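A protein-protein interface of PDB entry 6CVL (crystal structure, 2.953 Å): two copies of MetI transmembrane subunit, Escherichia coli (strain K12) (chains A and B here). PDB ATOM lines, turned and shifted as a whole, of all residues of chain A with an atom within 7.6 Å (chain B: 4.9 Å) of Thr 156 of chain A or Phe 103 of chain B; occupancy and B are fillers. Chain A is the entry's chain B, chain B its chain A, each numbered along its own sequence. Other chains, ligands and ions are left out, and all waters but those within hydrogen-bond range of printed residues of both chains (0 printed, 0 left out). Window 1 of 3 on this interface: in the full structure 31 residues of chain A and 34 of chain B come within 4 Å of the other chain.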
ATOM      1  N   THR A  20      25.887 -21.962  -9.614  1.00  0.00           N
ATOM      2  CA  THR A  20      25.395 -20.593  -9.569  1.00  0.00           C
ATOM      3  C   THR A  20      26.522 -19.595  -9.803  1.00  0.00           C
ATOM      4  O   THR A  20      26.476 -18.795 -10.744  1.00  0.00           O
ATOM      5  CB  THR A  20      24.713 -20.336  -8.226  1.00  0.00           C
ATOM      6  OG1 THR A  20      23.555 -21.175  -8.112  1.00  0.00           O
ATOM      7  CG2 THR A  20      24.306 -18.871  -8.098  1.00  0.00           C
ATOM      8  N   ARG A  64      18.035 -16.327 -26.661  1.00  0.00           N
ATOM      9  CA  ARG A  64      16.953 -16.260 -25.688  1.00  0.00           C
ATOM     10  C   ARG A  64      15.798 -17.180 -26.067  1.00  0.00           C
ATOM     11  O   ARG A  64      15.129 -17.728 -25.186  1.00  0.00           O
ATOM     12  CB  ARG A  64      16.469 -14.815 -25.555  1.00  0.00           C
ATOM     13  CG  ARG A  64      17.500 -13.873 -24.939  1.00  0.00           C
ATOM     14  CD  ARG A  64      17.241 -13.619 -23.460  1.00  0.00           C
ATOM     15  NE  ARG A  64      16.454 -12.407 -23.232  1.00  0.00           N
ATOM     16  CZ  ARG A  64      15.820 -12.124 -22.095  1.00  0.00           C
ATOM     17  NH1 ARG A  64      15.866 -12.967 -21.074  1.00  0.00           N
ATOM     18  NH2 ARG A  64      15.135 -10.995 -21.979  1.00  0.00           N
ATOM     19  N   ALA A 100      22.493 -18.151 -19.640  1.00  0.00           N
ATOM     20  CA  ALA A 100      22.376 -16.945 -18.833  1.00  0.00           C
ATOM     21  C   ALA A 100      22.939 -15.711 -19.529  1.00  0.00           C
ATOM     22  O   ALA A 100      22.410 -14.608 -19.341  1.00  0.00           O
ATOM     23  CB  ALA A 100      23.079 -17.147 -17.490  1.00  0.00           C
ATOM     24  N   PHE A 103      20.515 -12.955 -21.171  1.00  0.00           N
ATOM     25  CA  PHE A 103      19.754 -12.243 -20.156  1.00  0.00           C
ATOM     26  C   PHE A 103      20.642 -11.252 -19.417  1.00  0.00           C
ATOM     27  O   PHE A 103      20.237 -10.112 -19.162  1.00  0.00           O
ATOM     28  CB  PHE A 103      19.126 -13.254 -19.197  1.00  0.00           C
ATOM     29  CG  PHE A 103      18.639 -12.660 -17.907  1.00  0.00           C
ATOM     30  CD1 PHE A 103      17.382 -12.088 -17.821  1.00  0.00           C
ATOM     31  CD2 PHE A 103      19.432 -12.695 -16.774  1.00  0.00           C
ATOM     32  CE1 PHE A 103      16.934 -11.551 -16.635  1.00  0.00           C
ATOM     33  CE2 PHE A 103      18.987 -12.158 -15.584  1.00  0.00           C
ATOM     34  CZ  PHE A 103      17.737 -11.587 -15.515  1.00  0.00           C
ATOM     35  N   MET A 107      20.138  -7.231 -19.162  1.00  0.00           N
ATOM     36  CA  MET A 107      20.164  -6.523 -17.887  1.00  0.00           C
ATOM     37  C   MET A 107      21.200  -5.408 -17.907  1.00  0.00           C
ATOM     38  O   MET A 107      20.942  -4.292 -17.445  1.00  0.00           O
ATOM     39  CB  MET A 107      20.465  -7.500 -16.750  1.00  0.00           C
ATOM     40  CG  MET A 107      19.405  -8.572 -16.511  1.00  0.00           C
ATOM     41  SD  MET A 107      17.771  -7.944 -16.092  1.00  0.00           S
ATOM     42  CE  MET A 107      18.126  -6.918 -14.670  1.00  0.00           C
ATOM     43  N   ALA A 149      21.789  -5.803 -10.646  1.00  0.00           N
ATOM     44  CA  ALA A 149      21.470  -6.779 -11.675  1.00  0.00           C
ATOM     45  C   ALA A 149      22.148  -8.107 -11.381  1.00  0.00           C
ATOM     46  O   ALA A 149      21.533  -9.167 -11.514  1.00  0.00           O
ATOM     47  CB  ALA A 149      21.893  -6.255 -13.047  1.00  0.00           C
ATOM     48  N   ALA A 150      23.423  -8.066 -10.994  1.00  0.00           N
ATOM     49  CA  ALA A 150      24.131  -9.298 -10.667  1.00  0.00           C
ATOM     50  C   ALA A 150      23.458 -10.016  -9.508  1.00  0.00           C
ATOM     51  O   ALA A 150      23.317 -11.244  -9.521  1.00  0.00           O
ATOM     52  CB  ALA A 150      25.589  -8.992 -10.333  1.00  0.00           C
ATOM     53  N   THR A 151      23.051  -9.265  -8.486  1.00  0.00           N
ATOM     54  CA  THR A 151      22.294  -9.844  -7.386  1.00  0.00           C
ATOM     55  C   THR A 151      21.092 -10.609  -7.920  1.00  0.00           C
ATOM     56  O   THR A 151      20.932 -11.813  -7.673  1.00  0.00           O
ATOM     57  CB  THR A 151      21.845  -8.737  -6.432  1.00  0.00           C
ATOM     58  OG1 THR A 151      22.977  -7.955  -6.037  1.00  0.00           O
ATOM     59  CG2 THR A 151      21.177  -9.318  -5.200  1.00  0.00           C
ATOM     60  N   ILE A 152      20.239  -9.907  -8.669  1.00  0.00           N
ATOM     61  CA  ILE A 152      19.043 -10.521  -9.239  1.00  0.00           C
ATOM     62  C   ILE A 152      19.409 -11.787 -10.002  1.00  0.00           C
ATOM     63  O   ILE A 152      18.779 -12.845  -9.852  1.00  0.00           O
ATOM     64  CB  ILE A 152      18.320  -9.513 -10.151  1.00  0.00           C
ATOM     65  CG1 ILE A 152      17.850  -8.297  -9.352  1.00  0.00           C
ATOM     66  CG2 ILE A 152      17.142 -10.170 -10.845  1.00  0.00           C
ATOM     67  CD1 ILE A 152      17.655  -7.056 -10.201  1.00  0.00           C
ATOM     68  N   THR A 153      20.438 -11.691 -10.838  1.00  0.00           N
ATOM     69  CA  THR A 153      20.761 -12.771 -11.758  1.00  0.00           C
ATOM     70  C   THR A 153      21.238 -14.007 -11.009  1.00  0.00           C
ATOM     71  O   THR A 153      20.872 -15.130 -11.369  1.00  0.00           O
ATOM     72  CB  THR A 153      21.810 -12.298 -12.761  1.00  0.00           C
ATOM     73  OG1 THR A 153      21.263 -11.236 -13.557  1.00  0.00           O
ATOM     74  CG2 THR A 153      22.241 -13.438 -13.664  1.00  0.00           C
ATOM     75  N   LEU A 154      22.050 -13.831  -9.969  1.00  0.00           N
ATOM     76  CA  LEU A 154      22.497 -14.991  -9.207  1.00  0.00           C
ATOM     77  C   LEU A 154      21.342 -15.614  -8.433  1.00  0.00           C
ATOM     78  O   LEU A 154      21.236 -16.850  -8.340  1.00  0.00           O
ATOM     79  CB  LEU A 154      23.629 -14.595  -8.263  1.00  0.00           C
ATOM     80  CG  LEU A 154      24.962 -14.281  -8.944  1.00  0.00           C
ATOM     81  CD1 LEU A 154      25.849 -13.450  -8.030  1.00  0.00           C
ATOM     82  CD2 LEU A 154      25.668 -15.573  -9.361  1.00  0.00           C
ATOM     83  N   ILE A 155      20.460 -14.782  -7.868  1.00  0.00           N
ATOM     84  CA  ILE A 155      19.295 -15.341  -7.192  1.00  0.00           C
ATOM     85  C   ILE A 155      18.513 -16.222  -8.157  1.00  0.00           C
ATOM     86  O   ILE A 155      18.069 -17.318  -7.801  1.00  0.00           O
ATOM     87  CB  ILE A 155      18.406 -14.235  -6.599  1.00  0.00           C
ATOM     88  CG1 ILE A 155      19.195 -13.350  -5.634  1.00  0.00           C
ATOM     89  CG2 ILE A 155      17.225 -14.856  -5.863  1.00  0.00           C
ATOM     90  CD1 ILE A 155      19.825 -14.085  -4.478  1.00  0.00           C
ATOM     91  N   THR A 156      18.343 -15.763  -9.397  1.00  0.00           N
ATOM     92  CA  THR A 156      17.698 -16.609 -10.396  1.00  0.00           C
ATOM     93  C   THR A 156      18.519 -17.865 -10.663  1.00  0.00           C
ATOM     94  O   THR A 156      17.970 -18.973 -10.761  1.00  0.00           O
ATOM     95  CB  THR A 156      17.497 -15.833 -11.694  1.00  0.00           C
ATOM     96  OG1 THR A 156      18.642 -15.004 -11.926  1.00  0.00           O
ATOM     97  CG2 THR A 156      16.230 -14.985 -11.639  1.00  0.00           C
ATOM     98  N   LEU A 157      19.838 -17.710 -10.781  1.00  0.00           N
ATOM     99  CA  LEU A 157      20.688 -18.827 -11.162  1.00  0.00           C
ATOM    100  C   LEU A 157      20.612 -19.966 -10.155  1.00  0.00           C
ATOM    101  O   LEU A 157      20.843 -21.118 -10.519  1.00  0.00           O
ATOM    102  CB  LEU A 157      22.135 -18.362 -11.322  1.00  0.00           C
ATOM    103  CG  LEU A 157      22.538 -17.774 -12.676  1.00  0.00           C
ATOM    104  CD1 LEU A 157      24.042 -17.586 -12.751  1.00  0.00           C
ATOM    105  CD2 LEU A 157      22.078 -18.672 -13.810  1.00  0.00           C
ATOM    106  N   VAL A 158      20.284 -19.678  -8.896  1.00  0.00           N
ATOM    107  CA  VAL A 158      20.138 -20.776  -7.934  1.00  0.00           C
ATOM    108  C   VAL A 158      19.142 -21.810  -8.460  1.00  0.00           C
ATOM    109  O   VAL A 158      19.493 -22.965  -8.741  1.00  0.00           O
ATOM    110  CB  VAL A 158      19.708 -20.245  -6.557  1.00  0.00           C
ATOM    111  CG1 VAL A 158      19.506 -21.407  -5.582  1.00  0.00           C
ATOM    112  CG2 VAL A 158      20.739 -19.268  -6.018  1.00  0.00           C
ATOM    113  N   GLY A 159      17.883 -21.396  -8.625  1.00  0.00           N
ATOM    114  CA  GLY A 159      16.867 -22.306  -9.126  1.00  0.00           C
ATOM    115  C   GLY A 159      17.111 -22.751 -10.553  1.00  0.00           C
ATOM    116  O   GLY A 159      16.764 -23.879 -10.926  1.00  0.00           O
ATOM    117  N   TYR A 160      17.683 -21.875 -11.382  1.00  0.00           N
ATOM    118  CA  TYR A 160      17.958 -22.254 -12.763  1.00  0.00           C
ATOM    119  C   TYR A 160      18.956 -23.405 -12.820  1.00  0.00           C
ATOM    120  O   TYR A 160      18.802 -24.337 -13.620  1.00  0.00           O
ATOM    121  CB  TYR A 160      18.469 -21.037 -13.530  1.00  0.00           C
ATOM    122  CG  TYR A 160      18.392 -21.150 -15.035  1.00  0.00           C
ATOM    123  CD1 TYR A 160      17.241 -20.784 -15.723  1.00  0.00           C
ATOM    124  CD2 TYR A 160      19.478 -21.598 -15.770  1.00  0.00           C
ATOM    125  CE1 TYR A 160      17.175 -20.875 -17.103  1.00  0.00           C
ATOM    126  CE2 TYR A 160      19.421 -21.694 -17.146  1.00  0.00           C
ATOM    127  CZ  TYR A 160      18.270 -21.332 -17.807  1.00  0.00           C
ATOM    128  OH  TYR A 160      18.223 -21.428 -19.177  1.00  0.00           O
ATOM    129  N   SER A 161      19.980 -23.361 -11.966  1.00  0.00           N
ATOM    130  CA  SER A 161      20.911 -24.472 -11.838  1.00  0.00           C
ATOM    131  C   SER A 161      20.210 -25.696 -11.277  1.00  0.00           C
ATOM    132  O   SER A 161      20.438 -26.814 -11.744  1.00  0.00           O
ATOM    133  CB  SER A 161      22.080 -24.070 -10.941  1.00  0.00           C
ATOM    134  OG  SER A 161      21.663 -23.945  -9.592  1.00  0.00           O
ATOM    135  N   ALA A 162      19.362 -25.509 -10.265  1.00  0.00           N
ATOM    136  CA  ALA A 162      18.568 -26.627  -9.764  1.00  0.00           C
ATOM    137  C   ALA A 162      17.894 -27.373 -10.912  1.00  0.00           C
ATOM    138  O   ALA A 162      17.991 -28.601 -11.017  1.00  0.00           O
ATOM    139  CB  ALA A 162      17.529 -26.126  -8.762  1.00  0.00           C
ATOM    140  N   VAL A 200      19.930 -17.548  -0.687  1.00  0.00           N
ATOM    141  CA  VAL A 200      19.404 -16.344  -1.319  1.00  0.00           C
ATOM    142  C   VAL A 200      19.572 -15.154  -0.387  1.00  0.00           C
ATOM    143  O   VAL A 200      19.893 -14.043  -0.825  1.00  0.00           O
ATOM    144  CB  VAL A 200      17.934 -16.539  -1.730  1.00  0.00           C
ATOM    145  CG1 VAL A 200      17.816 -17.661  -2.745  1.00  0.00           C
ATOM    146  CG2 VAL A 200      17.059 -16.812  -0.522  1.00  0.00           C
ATOM    147  N   ILE A 203      23.139 -13.967  -0.570  1.00  0.00           N
ATOM    148  CA  ILE A 203      23.454 -13.303  -1.831  1.00  0.00           C
ATOM    149  C   ILE A 203      22.861 -11.898  -1.849  1.00  0.00           C
ATOM    150  O   ILE A 203      23.519 -10.930  -2.241  1.00  0.00           O
ATOM    151  CB  ILE A 203      22.957 -14.146  -3.013  1.00  0.00           C
ATOM    152  CG1 ILE A 203      23.619 -15.526  -2.994  1.00  0.00           C
ATOM    153  CG2 ILE A 203      23.268 -13.442  -4.318  1.00  0.00           C
ATOM    154  CD1 ILE A 203      22.836 -16.579  -3.739  1.00  0.00           C
ATOM    155  N   ARG B  64      11.437 -16.648  -3.762  1.00  0.00           N
ATOM    156  CA  ARG B  64      12.488 -16.829  -4.752  1.00  0.00           C
ATOM    157  C   ARG B  64      13.248 -18.129  -4.533  1.00  0.00           C
ATOM    158  O   ARG B  64      13.661 -18.779  -5.500  1.00  0.00           O
ATOM    159  CB  ARG B  64      13.440 -15.635  -4.710  1.00  0.00           C
ATOM    160  CG  ARG B  64      12.803 -14.328  -5.159  1.00  0.00           C
ATOM    161  CD  ARG B  64      13.151 -14.012  -6.603  1.00  0.00           C
ATOM    162  NE  ARG B  64      14.335 -13.164  -6.692  1.00  0.00           N
ATOM    163  CZ  ARG B  64      15.059 -13.000  -7.793  1.00  0.00           C
ATOM    164  NH1 ARG B  64      14.730 -13.634  -8.910  1.00  0.00           N
ATOM    165  NH2 ARG B  64      16.121 -12.204  -7.775  1.00  0.00           N
ATOM    166  N   GLY B  99       5.549 -17.815  -9.261  1.00  0.00           N
ATOM    167  CA  GLY B  99       6.992 -17.903  -9.383  1.00  0.00           C
ATOM    168  C   GLY B  99       7.611 -16.620  -9.895  1.00  0.00           C
ATOM    169  O   GLY B  99       8.680 -16.210  -9.439  1.00  0.00           O
ATOM    170  N   ALA B 100       6.943 -15.959 -10.837  1.00  0.00           N
ATOM    171  CA  ALA B 100       7.545 -14.790 -11.465  1.00  0.00           C
ATOM    172  C   ALA B 100       7.410 -13.527 -10.623  1.00  0.00           C
ATOM    173  O   ALA B 100       8.321 -12.692 -10.629  1.00  0.00           O
ATOM    174  CB  ALA B 100       6.924 -14.556 -12.843  1.00  0.00           C
ATOM    175  N   ALA B 101       6.308 -13.369  -9.891  1.00  0.00           N
ATOM    176  CA  ALA B 101       6.036 -12.090  -9.242  1.00  0.00           C
ATOM    177  C   ALA B 101       7.186 -11.557  -8.392  1.00  0.00           C
ATOM    178  O   ALA B 101       7.442 -10.343  -8.448  1.00  0.00           O
ATOM    179  CB  ALA B 101       4.761 -12.211  -8.394  1.00  0.00           C
ATOM    180  N   PRO B 102       7.900 -12.363  -7.599  1.00  0.00           N
ATOM    181  CA  PRO B 102       8.996 -11.790  -6.795  1.00  0.00           C
ATOM    182  C   PRO B 102      10.124 -11.240  -7.643  1.00  0.00           C
ATOM    183  O   PRO B 102      10.659 -10.159  -7.358  1.00  0.00           O
ATOM    184  CB  PRO B 102       9.467 -12.976  -5.940  1.00  0.00           C
ATOM    185  CG  PRO B 102       8.368 -13.972  -5.997  1.00  0.00           C
ATOM    186  CD  PRO B 102       7.699 -13.792  -7.320  1.00  0.00           C
ATOM    187  N   PHE B 103      10.520 -11.979  -8.674  1.00  0.00           N
ATOM    188  CA  PHE B 103      11.514 -11.462  -9.599  1.00  0.00           C
ATOM    189  C   PHE B 103      11.043 -10.152 -10.215  1.00  0.00           C
ATOM    190  O   PHE B 103      11.822  -9.198 -10.344  1.00  0.00           O
ATOM    191  CB  PHE B 103      11.793 -12.501 -10.679  1.00  0.00           C
ATOM    192  CG  PHE B 103      12.491 -11.949 -11.880  1.00  0.00           C
ATOM    193  CD1 PHE B 103      13.866 -11.825 -11.901  1.00  0.00           C
ATOM    194  CD2 PHE B 103      11.772 -11.559 -12.991  1.00  0.00           C
ATOM    195  CE1 PHE B 103      14.511 -11.317 -13.008  1.00  0.00           C
ATOM    196  CE2 PHE B 103      12.411 -11.052 -14.101  1.00  0.00           C
ATOM    197  CZ  PHE B 103      13.782 -10.931 -14.108  1.00  0.00           C
ATOM    198  N   ILE B 104       9.769 -10.091 -10.605  1.00  0.00           N
ATOM    199  CA  ILE B 104       9.208  -8.854 -11.138  1.00  0.00           C
ATOM    200  C   ILE B 104       9.370  -7.725 -10.133  1.00  0.00           C
ATOM    201  O   ILE B 104       9.741  -6.599 -10.491  1.00  0.00           O
ATOM    202  CB  ILE B 104       7.727  -9.059 -11.509  1.00  0.00           C
ATOM    203  CG1 ILE B 104       7.596 -10.020 -12.689  1.00  0.00           C
ATOM    204  CG2 ILE B 104       7.077  -7.721 -11.825  1.00  0.00           C
ATOM    205  CD1 ILE B 104       6.190 -10.543 -12.893  1.00  0.00           C
ATOM    206  N   ALA B 105       9.076  -8.001  -8.862  1.00  0.00           N
ATOM    207  CA  ALA B 105       9.171  -6.964  -7.844  1.00  0.00           C
ATOM    208  C   ALA B 105      10.602  -6.472  -7.695  1.00  0.00           C
ATOM    209  O   ALA B 105      10.837  -5.271  -7.525  1.00  0.00           O
ATOM    210  CB  ALA B 105       8.646  -7.493  -6.512  1.00  0.00           C
ATOM    211  N   ARG B 106      11.574  -7.384  -7.742  1.00  0.00           N
ATOM    212  CA  ARG B 106      12.964  -6.955  -7.621  1.00  0.00           C
ATOM    213  C   ARG B 106      13.382  -6.126  -8.826  1.00  0.00           C
ATOM    214  O   ARG B 106      14.110  -5.136  -8.681  1.00  0.00           O
ATOM    215  CB  ARG B 106      13.890  -8.155  -7.449  1.00  0.00           C
ATOM    216  CG  ARG B 106      13.880  -8.744  -6.044  1.00  0.00           C
ATOM    217  CD  ARG B 106      14.486  -7.781  -5.023  1.00  0.00           C
ATOM    218  NE  ARG B 106      14.798  -8.452  -3.763  1.00  0.00           N
ATOM    219  CZ  ARG B 106      14.896  -7.843  -2.584  1.00  0.00           C
ATOM    220  NH1 ARG B 106      14.699  -6.535  -2.481  1.00  0.00           N
ATOM    221  NH2 ARG B 106      15.187  -8.548  -1.503  1.00  0.00           N
ATOM    222  N   MET B 107      12.937  -6.517 -10.022  1.00  0.00           N
ATOM    223  CA  MET B 107      13.183  -5.699 -11.205  1.00  0.00           C
ATOM    224  C   MET B 107      12.607  -4.301 -11.020  1.00  0.00           C
ATOM    225  O   MET B 107      13.261  -3.298 -11.337  1.00  0.00           O
ATOM    226  CB  MET B 107      12.576  -6.373 -12.433  1.00  0.00           C
ATOM    227  CG  MET B 107      13.227  -7.698 -12.818  1.00  0.00           C
ATOM    228  SD  MET B 107      14.962  -7.571 -13.290  1.00  0.00           S
ATOM    229  CE  MET B 107      14.861  -6.398 -14.640  1.00  0.00           C
ATOM    230  N   THR B 153      11.240  -9.610 -18.890  1.00  0.00           N
ATOM    231  CA  THR B 153      10.523 -10.608 -18.111  1.00  0.00           C
ATOM    232  C   THR B 153       9.689 -11.510 -19.004  1.00  0.00           C
ATOM    233  O   THR B 153       9.647 -12.726 -18.799  1.00  0.00           O
ATOM    234  CB  THR B 153       9.639  -9.906 -17.079  1.00  0.00           C
ATOM    235  OG1 THR B 153      10.464  -9.168 -16.169  1.00  0.00           O
ATOM    236  CG2 THR B 153       8.794 -10.910 -16.301  1.00  0.00           C
ATOM    237  N   THR B 156      11.817 -13.962 -20.863  1.00  0.00           N
ATOM    238  CA  THR B 156      12.092 -15.106 -19.993  1.00  0.00           C
ATOM    239  C   THR B 156      10.872 -16.019 -19.876  1.00  0.00           C
ATOM    240  O   THR B 156      10.992 -17.253 -19.931  1.00  0.00           O
ATOM    241  CB  THR B 156      12.520 -14.632 -18.606  1.00  0.00           C
ATOM    242  OG1 THR B 156      11.735 -13.495 -18.228  1.00  0.00           O
ATOM    243  CG2 THR B 156      14.002 -14.269 -18.583  1.00  0.00           C
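Among the printed residues, merely in contact across the chains: Ile 155 of chain A with Arg 64 of chain B (3.3 Å), Met 107 of chain A with Met 107 of chain B (3.3 Å), Arg 64 of chain A with Thr 156 of chain B (3.4 Å), Thr 156 of chain A with Arg 64 of chain B (3.4 Å), Ile 152 of chain A with Phe 103 of chain B (3.6 Å) and Thr 156 of chain A with Phe 103 of chain B (3.96 Å).
The backbone carbonyl oxygen (O) of Ile 152 of chain A is in hydrogen-bond range of the guanidinium group (NH2) of Arg 64 of chain B, at 3.4 Å.
The backbone carbonyl oxygen (O) of Ile 152 of chain A sits at hydrogen-bond distance from the side-chain hydroxyl (OG1) of Thr 156 of chain A (3.0 Å).
Phe 103 of chain B touches just these residues of chain A: Ile 152 (3.6 Å) and Thr 156 (3.96 Å). Of the printed residues of chain B, Ile 152 of chain A touches Arg 64 and Phe 103. Of the printed residues of chain B, Met 107 of chain A touches Met 107 (3.3 Å). Val 200 of chain A touches none of the printed residues of chain B. Phe 103 of chain A touches none of the printed residues of chain B.
Hydrophobic or aromatic side chains of chain A that line the printed part of chain B: Met 107, Ile 152 and Ile 155. Printed residues of chain B that touch a printed residue of chain A: Arg 64, Phe 103, Met 107 and Thr 156. Hydrophobic or aromatic side chains of chain B that line the printed part of chain A: Phe 103 and Met 107. Along chain B the printed residues that touch a printed residue of chain A span positions 64 to 156.
Arg 64 of chain A touches Thr 156 of chain B, and with the chains exchanged Thr 156 of chain A touches Arg 64 of chain B. Met 107 of chain A touches its own counterpart, Met 107 of chain B. Thr 156 of chain A touches Phe 103 of chain B, but with the chains exchanged Phe 103 of chain A does not touch Thr 156 of chain B (4.1 Å). Positions printed for both chains: 64, 100, 103, 107, 153 and 156. Of the 7 pairs that touch across the chains among the printed residues, 3 have their exchanged pair printed and touching as well.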
